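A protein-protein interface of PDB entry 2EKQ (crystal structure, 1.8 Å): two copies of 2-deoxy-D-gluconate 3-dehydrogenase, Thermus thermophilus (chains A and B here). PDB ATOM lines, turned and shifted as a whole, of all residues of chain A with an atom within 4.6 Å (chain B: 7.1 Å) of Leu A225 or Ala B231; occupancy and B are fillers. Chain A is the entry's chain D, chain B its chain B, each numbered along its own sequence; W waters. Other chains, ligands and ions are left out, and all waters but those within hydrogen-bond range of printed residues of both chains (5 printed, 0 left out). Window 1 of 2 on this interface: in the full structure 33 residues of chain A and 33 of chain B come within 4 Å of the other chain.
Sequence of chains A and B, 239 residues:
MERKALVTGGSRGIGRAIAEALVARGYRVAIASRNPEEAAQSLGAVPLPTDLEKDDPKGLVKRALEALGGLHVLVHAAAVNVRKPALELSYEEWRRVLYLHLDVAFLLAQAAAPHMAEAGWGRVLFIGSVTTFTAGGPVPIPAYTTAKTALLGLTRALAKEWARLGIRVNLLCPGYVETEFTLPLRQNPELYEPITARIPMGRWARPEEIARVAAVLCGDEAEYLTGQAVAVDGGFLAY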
ATOM      1  N   ARG A 168     -10.862  19.323 -19.301  1.00  0.00           N
ATOM      2  CA  ARG A 168     -11.908  18.361 -19.632  1.00  0.00           C
ATOM      3  C   ARG A 168     -12.043  17.477 -18.402  1.00  0.00           C
ATOM      4  O   ARG A 168     -11.038  17.088 -17.802  1.00  0.00           O
ATOM      5  CB  ARG A 168     -11.513  17.517 -20.847  1.00  0.00           C
ATOM      6  CG  ARG A 168     -11.115  18.343 -22.063  1.00  0.00           C
ATOM      7  CD  ARG A 168     -12.271  19.191 -22.577  1.00  0.00           C
ATOM      8  NE  ARG A 168     -11.824  20.131 -23.601  1.00  0.00           N
ATOM      9  CZ  ARG A 168     -11.754  21.448 -23.434  1.00  0.00           C
ATOM     10  NH1 ARG A 168     -12.106  21.997 -22.279  1.00  0.00           N
ATOM     11  NH2 ARG A 168     -11.320  22.222 -24.422  1.00  0.00           N
ATOM     12  N   ASN A 170     -13.955  13.969 -16.998  1.00  0.00           N
ATOM     13  CA  ASN A 170     -14.741  12.790 -17.335  1.00  0.00           C
ATOM     14  C   ASN A 170     -14.660  11.700 -16.276  1.00  0.00           C
ATOM     15  O   ASN A 170     -13.814  11.740 -15.377  1.00  0.00           O
ATOM     16  CB  ASN A 170     -14.295  12.240 -18.689  1.00  0.00           C
ATOM     17  CG  ASN A 170     -14.584  13.204 -19.830  1.00  0.00           C
ATOM     18  OD1 ASN A 170     -15.743  13.454 -20.169  1.00  0.00           O
ATOM     19  ND2 ASN A 170     -13.534  13.751 -20.425  1.00  0.00           N
ATOM     20  N   LEU A 217      -8.793   9.522 -22.449  1.00  0.00           N
ATOM     21  CA  LEU A 217      -9.473  10.587 -21.730  1.00  0.00           C
ATOM     22  C   LEU A 217      -8.492  11.553 -21.067  1.00  0.00           C
ATOM     23  O   LEU A 217      -8.898  12.587 -20.530  1.00  0.00           O
ATOM     24  CB  LEU A 217     -10.423   9.977 -20.694  1.00  0.00           C
ATOM     25  CG  LEU A 217     -11.535   9.111 -21.301  1.00  0.00           C
ATOM     26  CD1 LEU A 217     -12.328   8.424 -20.195  1.00  0.00           C
ATOM     27  CD2 LEU A 217     -12.456   9.984 -22.156  1.00  0.00           C
ATOM     28  N   ALA A 222      -9.570  13.679 -26.272  1.00  0.00           N
ATOM     29  CA  ALA A 222     -10.727  14.175 -25.531  1.00  0.00           C
ATOM     30  C   ALA A 222     -10.900  15.690 -25.607  1.00  0.00           C
ATOM     31  O   ALA A 222     -11.553  16.288 -24.751  1.00  0.00           O
ATOM     32  CB  ALA A 222     -10.627  13.737 -24.069  1.00  0.00           C
ATOM     33  N   GLU A 223     -10.330  16.307 -26.639  1.00  0.00           N
ATOM     34  CA  GLU A 223     -10.424  17.756 -26.819  1.00  0.00           C
ATOM     35  C   GLU A 223     -11.859  18.295 -26.797  1.00  0.00           C
ATOM     36  O   GLU A 223     -12.104  19.387 -26.279  1.00  0.00           O
ATOM     37  CB  GLU A 223      -9.718  18.157 -28.124  1.00  0.00           C
ATOM     38  CG  GLU A 223      -9.974  19.587 -28.619  1.00  0.00           C
ATOM     39  CD  GLU A 223      -9.660  20.660 -27.590  1.00  0.00           C
ATOM     40  OE1 GLU A 223      -8.820  20.418 -26.696  1.00  0.00           O
ATOM     41  OE2 GLU A 223     -10.245  21.764 -27.688  1.00  0.00           O
ATOM     42  N   TYR A 224     -12.806  17.536 -27.344  1.00  0.00           N
ATOM     43  CA  TYR A 224     -14.202  17.972 -27.368  1.00  0.00           C
ATOM     44  C   TYR A 224     -15.075  16.996 -26.577  1.00  0.00           C
ATOM     45  O   TYR A 224     -16.291  16.943 -26.764  1.00  0.00           O
ATOM     46  CB  TYR A 224     -14.708  18.057 -28.815  1.00  0.00           C
ATOM     47  CG  TYR A 224     -15.874  19.008 -29.017  1.00  0.00           C
ATOM     48  CD1 TYR A 224     -15.684  20.390 -28.983  1.00  0.00           C
ATOM     49  CD2 TYR A 224     -17.164  18.528 -29.233  1.00  0.00           C
ATOM     50  CE1 TYR A 224     -16.752  21.272 -29.163  1.00  0.00           C
ATOM     51  CE2 TYR A 224     -18.240  19.398 -29.408  1.00  0.00           C
ATOM     52  CZ  TYR A 224     -18.027  20.767 -29.373  1.00  0.00           C
ATOM     53  OH  TYR A 224     -19.088  21.624 -29.555  1.00  0.00           O
ATOM     54  N   LEU A 225     -14.447  16.218 -25.699  1.00  0.00           N
ATOM     55  CA  LEU A 225     -15.164  15.240 -24.887  1.00  0.00           C
ATOM     56  C   LEU A 225     -15.045  15.617 -23.412  1.00  0.00           C
ATOM     57  O   LEU A 225     -13.959  15.556 -22.826  1.00  0.00           O
ATOM     58  CB  LEU A 225     -14.579  13.840 -25.117  1.00  0.00           C
ATOM     59  CG  LEU A 225     -15.442  12.621 -24.776  1.00  0.00           C
ATOM     60  CD1 LEU A 225     -14.717  11.360 -25.225  1.00  0.00           C
ATOM     61  CD2 LEU A 225     -15.731  12.566 -23.280  1.00  0.00           C
ATOM     62  N   THR A 226     -16.159  16.012 -22.803  1.00  0.00           N
ATOM     63  CA  THR A 226     -16.130  16.400 -21.403  1.00  0.00           C
ATOM     64  C   THR A 226     -17.502  16.273 -20.742  1.00  0.00           C
ATOM     65  O   THR A 226     -18.533  16.384 -21.403  1.00  0.00           O
ATOM     66  CB  THR A 226     -15.600  17.853 -21.259  1.00  0.00           C
ATOM     67  OG1 THR A 226     -15.333  18.138 -19.881  1.00  0.00           O
ATOM     68  CG2 THR A 226     -16.613  18.856 -21.799  1.00  0.00           C
ATOM     69  N   GLN A 228     -18.690  13.565 -19.355  1.00  0.00           N
ATOM     70  CA  GLN A 228     -19.263  12.259 -19.653  1.00  0.00           C
ATOM     71  C   GLN A 228     -18.673  11.086 -18.884  1.00  0.00           C
ATOM     72  O   GLN A 228     -17.552  11.146 -18.385  1.00  0.00           O
ATOM     73  CB  GLN A 228     -19.109  11.967 -21.147  1.00  0.00           C
ATOM     74  CG  GLN A 228     -19.981  12.825 -22.038  1.00  0.00           C
ATOM     75  CD  GLN A 228     -21.447  12.542 -21.822  1.00  0.00           C
ATOM     76  OE1 GLN A 228     -21.867  11.385 -21.818  1.00  0.00           O
ATOM     77  NE2 GLN A 228     -22.234  13.594 -21.645  1.00  0.00           N
ATOM     78  N   SER B 129     -26.175  10.925 -31.860  1.00  0.00           N
ATOM     79  CA  SER B 129     -26.348  12.368 -31.903  1.00  0.00           C
ATOM     80  C   SER B 129     -26.750  12.857 -30.523  1.00  0.00           C
ATOM     81  O   SER B 129     -26.987  12.056 -29.622  1.00  0.00           O
ATOM     82  CB  SER B 129     -27.451  12.694 -32.918  1.00  0.00           C
ATOM     83  OG  SER B 129     -27.938  14.014 -32.777  1.00  0.00           O
ATOM     84  N   VAL B 130     -26.803  14.170 -30.338  1.00  0.00           N
ATOM     85  CA  VAL B 130     -27.244  14.679 -29.053  1.00  0.00           C
ATOM     86  C   VAL B 130     -28.713  14.288 -28.950  1.00  0.00           C
ATOM     87  O   VAL B 130     -29.267  14.212 -27.855  1.00  0.00           O
ATOM     88  CB  VAL B 130     -27.117  16.222 -28.953  1.00  0.00           C
ATOM     89  CG1 VAL B 130     -25.652  16.611 -28.849  1.00  0.00           C
ATOM     90  CG2 VAL B 130     -27.767  16.880 -30.155  1.00  0.00           C
ATOM     91  N   PHE B 133     -30.186  11.411 -26.853  1.00  0.00           N
ATOM     92  CA  PHE B 133     -30.524  11.670 -25.456  1.00  0.00           C
ATOM     93  C   PHE B 133     -31.489  12.830 -25.215  1.00  0.00           C
ATOM     94  O   PHE B 133     -31.964  13.021 -24.091  1.00  0.00           O
ATOM     95  CB  PHE B 133     -29.234  11.918 -24.675  1.00  0.00           C
ATOM     96  CG  PHE B 133     -28.264  10.781 -24.756  1.00  0.00           C
ATOM     97  CD1 PHE B 133     -28.472   9.621 -24.016  1.00  0.00           C
ATOM     98  CD2 PHE B 133     -27.159  10.852 -25.599  1.00  0.00           C
ATOM     99  CE1 PHE B 133     -27.595   8.544 -24.117  1.00  0.00           C
ATOM    100  CE2 PHE B 133     -26.275   9.779 -25.709  1.00  0.00           C
ATOM    101  CZ  PHE B 133     -26.496   8.623 -24.963  1.00  0.00           C
ATOM    102  N   LEU B 171     -21.710   3.297 -30.078  1.00  0.00           N
ATOM    103  CA  LEU B 171     -22.405   4.424 -30.683  1.00  0.00           C
ATOM    104  C   LEU B 171     -21.713   5.748 -30.367  1.00  0.00           C
ATOM    105  O   LEU B 171     -21.753   6.223 -29.234  1.00  0.00           O
ATOM    106  CB  LEU B 171     -23.850   4.472 -30.175  1.00  0.00           C
ATOM    107  CG  LEU B 171     -24.784   5.539 -30.756  1.00  0.00           C
ATOM    108  CD1 LEU B 171     -25.097   5.221 -32.213  1.00  0.00           C
ATOM    109  CD2 LEU B 171     -26.069   5.583 -29.936  1.00  0.00           C
ATOM    110  N   LEU B 172     -21.073   6.337 -31.370  1.00  0.00           N
ATOM    111  CA  LEU B 172     -20.405   7.620 -31.189  1.00  0.00           C
ATOM    112  C   LEU B 172     -21.474   8.691 -31.333  1.00  0.00           C
ATOM    113  O   LEU B 172     -22.159   8.754 -32.352  1.00  0.00           O
ATOM    114  CB  LEU B 172     -19.323   7.827 -32.251  1.00  0.00           C
ATOM    115  CG  LEU B 172     -18.636   9.199 -32.256  1.00  0.00           C
ATOM    116  CD1 LEU B 172     -17.897   9.418 -30.943  1.00  0.00           C
ATOM    117  CD2 LEU B 172     -17.667   9.274 -33.429  1.00  0.00           C
ATOM    118  N   CYS B 173     -21.618   9.530 -30.313  1.00  0.00           N
ATOM    119  CA  CYS B 173     -22.628  10.578 -30.344  1.00  0.00           C
ATOM    120  C   CYS B 173     -22.000  11.964 -30.398  1.00  0.00           C
ATOM    121  O   CYS B 173     -21.628  12.536 -29.374  1.00  0.00           O
ATOM    122  CB  CYS B 173     -23.539  10.456 -29.118  1.00  0.00           C
ATOM    123  SG  CYS B 173     -24.494   8.911 -29.057  1.00  0.00           S
ATOM    124  N   PRO B 174     -21.866  12.522 -31.609  1.00  0.00           N
ATOM    125  CA  PRO B 174     -21.275  13.851 -31.759  1.00  0.00           C
ATOM    126  C   PRO B 174     -22.227  14.909 -31.235  1.00  0.00           C
ATOM    127  O   PRO B 174     -23.443  14.695 -31.187  1.00  0.00           O
ATOM    128  CB  PRO B 174     -21.081  13.984 -33.273  1.00  0.00           C
ATOM    129  CG  PRO B 174     -21.111  12.558 -33.774  1.00  0.00           C
ATOM    130  CD  PRO B 174     -22.176  11.941 -32.923  1.00  0.00           C
ATOM    131  N   GLY B 175     -21.670  16.047 -30.842  1.00  0.00           N
ATOM    132  CA  GLY B 175     -22.499  17.133 -30.375  1.00  0.00           C
ATOM    133  C   GLY B 175     -22.840  17.963 -31.595  1.00  0.00           C
ATOM    134  O   GLY B 175     -23.212  17.420 -32.640  1.00  0.00           O
ATOM    135  N   MET B 201     -18.010  24.466 -23.727  1.00  0.00           N
ATOM    136  CA  MET B 201     -16.807  24.887 -24.438  1.00  0.00           C
ATOM    137  C   MET B 201     -17.035  26.149 -25.272  1.00  0.00           C
ATOM    138  O   MET B 201     -16.087  26.746 -25.784  1.00  0.00           O
ATOM    139  CB  MET B 201     -16.270  23.738 -25.298  1.00  0.00           C
ATOM    140  CG  MET B 201     -15.448  22.744 -24.475  1.00  0.00           C
ATOM    141  SD  MET B 201     -14.748  21.397 -25.430  1.00  0.00           S
ATOM    142  CE  MET B 201     -13.633  22.291 -26.531  1.00  0.00           C
ATOM    143  N   GLU B 209     -12.254  16.783 -34.728  1.00  0.00           N
ATOM    144  CA  GLU B 209     -12.249  16.614 -33.279  1.00  0.00           C
ATOM    145  C   GLU B 209     -13.140  15.438 -32.884  1.00  0.00           C
ATOM    146  O   GLU B 209     -12.886  14.757 -31.890  1.00  0.00           O
ATOM    147  CB  GLU B 209     -12.720  17.901 -32.597  1.00  0.00           C
ATOM    148  CG  GLU B 209     -11.736  19.053 -32.759  1.00  0.00           C
ATOM    149  CD  GLU B 209     -12.233  20.348 -32.157  1.00  0.00           C
ATOM    150  OE1 GLU B 209     -13.355  20.774 -32.502  1.00  0.00           O
ATOM    151  OE2 GLU B 209     -11.497  20.944 -31.343  1.00  0.00           O
ATOM    152  N   VAL B 213     -12.097  10.516 -31.582  1.00  0.00           N
ATOM    153  CA  VAL B 213     -12.727   9.525 -30.717  1.00  0.00           C
ATOM    154  C   VAL B 213     -13.228   8.345 -31.539  1.00  0.00           C
ATOM    155  O   VAL B 213     -13.170   7.199 -31.093  1.00  0.00           O
ATOM    156  CB  VAL B 213     -13.902  10.149 -29.925  1.00  0.00           C
ATOM    157  CG1 VAL B 213     -14.516   9.118 -28.984  1.00  0.00           C
ATOM    158  CG2 VAL B 213     -13.402  11.353 -29.138  1.00  0.00           C
ATOM    159  N   ALA B 229     -22.595   4.115 -25.620  1.00  0.00           N
ATOM    160  CA  ALA B 229     -22.696   5.350 -26.380  1.00  0.00           C
ATOM    161  C   ALA B 229     -21.609   6.229 -25.779  1.00  0.00           C
ATOM    162  O   ALA B 229     -21.437   6.261 -24.558  1.00  0.00           O
ATOM    163  CB  ALA B 229     -24.063   6.000 -26.183  1.00  0.00           C
ATOM    164  N   VAL B 230     -20.855   6.913 -26.631  1.00  0.00           N
ATOM    165  CA  VAL B 230     -19.802   7.801 -26.161  1.00  0.00           C
ATOM    166  C   VAL B 230     -20.113   9.165 -26.765  1.00  0.00           C
ATOM    167  O   VAL B 230     -20.045   9.342 -27.978  1.00  0.00           O
ATOM    168  CB  VAL B 230     -18.413   7.319 -26.633  1.00  0.00           C
ATOM    169  CG1 VAL B 230     -17.338   8.303 -26.199  1.00  0.00           C
ATOM    170  CG2 VAL B 230     -18.123   5.938 -26.051  1.00  0.00           C
ATOM    171  N   ALA B 231     -20.478  10.118 -25.914  1.00  0.00           N
ATOM    172  CA  ALA B 231     -20.821  11.452 -26.385  1.00  0.00           C
ATOM    173  C   ALA B 231     -19.622  12.389 -26.399  1.00  0.00           C
ATOM    174  O   ALA B 231     -18.929  12.548 -25.394  1.00  0.00           O
ATOM    175  CB  ALA B 231     -21.931  12.036 -25.519  1.00  0.00           C
ATOM    176  N   VAL B 232     -19.385  13.001 -27.556  1.00  0.00           N
ATOM    177  CA  VAL B 232     -18.285  13.945 -27.748  1.00  0.00           C
ATOM    178  C   VAL B 232     -19.019  15.224 -28.156  1.00  0.00           C
ATOM    179  O   VAL B 232     -19.225  15.489 -29.343  1.00  0.00           O
ATOM    180  CB  VAL B 232     -17.349  13.457 -28.879  1.00  0.00           C
ATOM    181  CG1 VAL B 232     -16.101  14.322 -28.943  1.00  0.00           C
ATOM    182  CG2 VAL B 232     -16.968  11.996 -28.634  1.00  0.00           C
ATOM    183  N   ASP B 233     -19.410  16.012 -27.159  1.00  0.00           N
ATOM    184  CA  ASP B 233     -20.212  17.208 -27.400  1.00  0.00           C
ATOM    185  C   ASP B 233     -19.793  18.510 -26.718  1.00  0.00           C
ATOM    186  O   ASP B 233     -20.629  19.402 -26.547  1.00  0.00           O
ATOM    187  CB  ASP B 233     -21.646  16.908 -26.983  1.00  0.00           C
ATOM    188  CG  ASP B 233     -21.759  16.626 -25.490  1.00  0.00           C
ATOM    189  OD1 ASP B 233     -20.726  16.727 -24.788  1.00  0.00           O
ATOM    190  OD2 ASP B 233     -22.867  16.311 -25.013  1.00  0.00           O
ATOM    191  N   GLY B 234     -18.532  18.626 -26.316  1.00  0.00           N
ATOM    192  CA  GLY B 234     -18.085  19.851 -25.672  1.00  0.00           C
ATOM    193  C   GLY B 234     -18.806  20.194 -24.377  1.00  0.00           C
ATOM    194  O   GLY B 234     -18.747  21.339 -23.915  1.00  0.00           O
ATOM    195  N   GLY B 235     -19.495  19.212 -23.797  1.00  0.00           N
ATOM    196  CA  GLY B 235     -20.196  19.427 -22.540  1.00  0.00           C
ATOM    197  C   GLY B 235     -21.686  19.704 -22.634  1.00  0.00           C
ATOM    198  O   GLY B 235     -22.350  19.879 -21.611  1.00  0.00           O
ATOM    199  N   LEU B 237     -24.553  17.909 -23.263  1.00  0.00           N
ATOM    200  CA  LEU B 237     -25.471  17.082 -22.489  1.00  0.00           C
ATOM    201  C   LEU B 237     -25.330  17.240 -20.976  1.00  0.00           C
ATOM    202  O   LEU B 237     -26.317  17.144 -20.246  1.00  0.00           O
ATOM    203  CB  LEU B 237     -25.300  15.615 -22.882  1.00  0.00           C
ATOM    204  CG  LEU B 237     -25.733  15.315 -24.322  1.00  0.00           C
ATOM    205  CD1 LEU B 237     -25.347  13.895 -24.698  1.00  0.00           C
ATOM    206  CD2 LEU B 237     -27.235  15.526 -24.460  1.00  0.00           C
HETATM  207  O   HOH W   1     -12.428  15.225 -29.097  1.00  0.00           O
HETATM  208  O   HOH W   2     -21.429  16.369 -22.057  1.00  0.00           O
HETATM  209  O   HOH W   3     -20.438   9.316 -23.060  1.00  0.00           O
HETATM  210  O   HOH W   4     -21.654  20.312 -29.023  1.00  0.00           O
HETATM  211  O   HOH W   5     -18.505  15.167 -24.486  1.00  0.00           O
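N of Gly B234 is in hydrogen-bond range of O of Tyr A224, 2.8 Å away.
N of Asp B233 is in hydrogen-bond range of O of Tyr A224, 3.3 Å away.
SD of Met B201 lies close to NH2 of Arg A168 (3.7 Å).
The backbone carbonyl oxygen (O) of Glu A223 sits close to the side-chain sulfur (SD) of Met B201 (3.4 Å).
N of Gly B175 sits at hydrogen-bond distance from O of Val B232, at 2.9 Å.
OE2 of Glu A223 lies within salt-bridge range of NH2 of Arg A168 (3.5 Å).
OD1 of Asn A170 lies within hydrogen-bond range of N of Gln A228, 3.1 Å away.
The side-chain carboxylate (OD2) of Asp B233 is in hydrogen-bond range of the backbone NH (N) of Leu B237 (2.9 Å).
The backbone NH (N) of Met B201 sits at hydrogen-bond distance from the backbone carbonyl oxygen (O) of Gly B234.
O of Cys B173 is in hydrogen-bond range of N of Val B232, 2.9 Å away.
Among the printed residues, merely in contact across the chains: Glu A223 with Glu B209, Tyr A224 with Met B201, Tyr A224 with Val B232, Leu A225 with Ala B231, Thr A226 with Gly B234, Thr A226 with Gly B235, Gln A228 with Ala B231 and Gln A228 with Leu B237.
Of chain B, only Ala B231 (3.5 Å) comes within 4 Å of Leu A225.
Of chain A, only Leu A225 and Gln A228 come within 4 Å of Ala B231.
Of the printed residues of chain B, Gln A228 touches Ala B231 (3.5 Å) and Leu B237 (3.9 Å).
Of the printed residues of chain B, Thr A226 touches Gly B234 and Gly B235.
Printed residues of chain B within 4 Å of Glu A223: Met B201 (3.3 Å) and Glu B209 (3.4 Å).
Of the printed residues of chain B, Arg A168 touches Met B201.
Of the printed residues of chain A, Asp B233 touches Tyr A224 (3.2 Å).
The nearest printed residue of chain A that does not touch Ala B231 is Thr A226 (5.1 Å).
The nearest printed residue of chain A that does not touch Val B232 is Leu A225 (4.1 Å).
Of the 9 printed residues of chain A, 6 touch a printed residue of chain B.
Hydrophobic or aromatic side chains of chain A within 4 Å of the printed part of chain B: Tyr A224 and Leu A225.
Hydrophobic or aromatic side chains of chain B that line the printed part of chain A: Met B201, Ala B231, Val B232 and Leu B237.
Among the printed residues, no Asp or Glu carboxylate lies within 4 Å of a Lys or Arg side-chain nitrogen of the other chain.
No position is printed for both chains.
Of the 12 pairs that touch across the chains among the printed residues, none has its exchanged pair printed and touching as well.
Water W5 lies within hydrogen-bond range of OD1 of Asp B233 (2.7 Å), O of Ala B231 (2.8 Å) and N of Thr A226 (3.0 Å).
Water W3 lies within hydrogen-bond range of the side-chain amide oxygen (OE1) of Gln A228 and the backbone NH (N) of Ala B231.
Water W4 bridges the backbone carbonyl oxygen of Asp B233 (2.8 Å) and the side-chain hydroxyl of Tyr A224 (2.9 Å).
Water W2 lies within hydrogen-bond range of the side-chain carboxylate (OD1) of Asp B233, the side-chain amide nitrogen (NE2) of Gln A228 and the backbone carbonyl oxygen (O) of Thr A226.
Water W1 lies within hydrogen-bond range of O of Glu B209, N of Tyr A224 and N of Glu A223.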
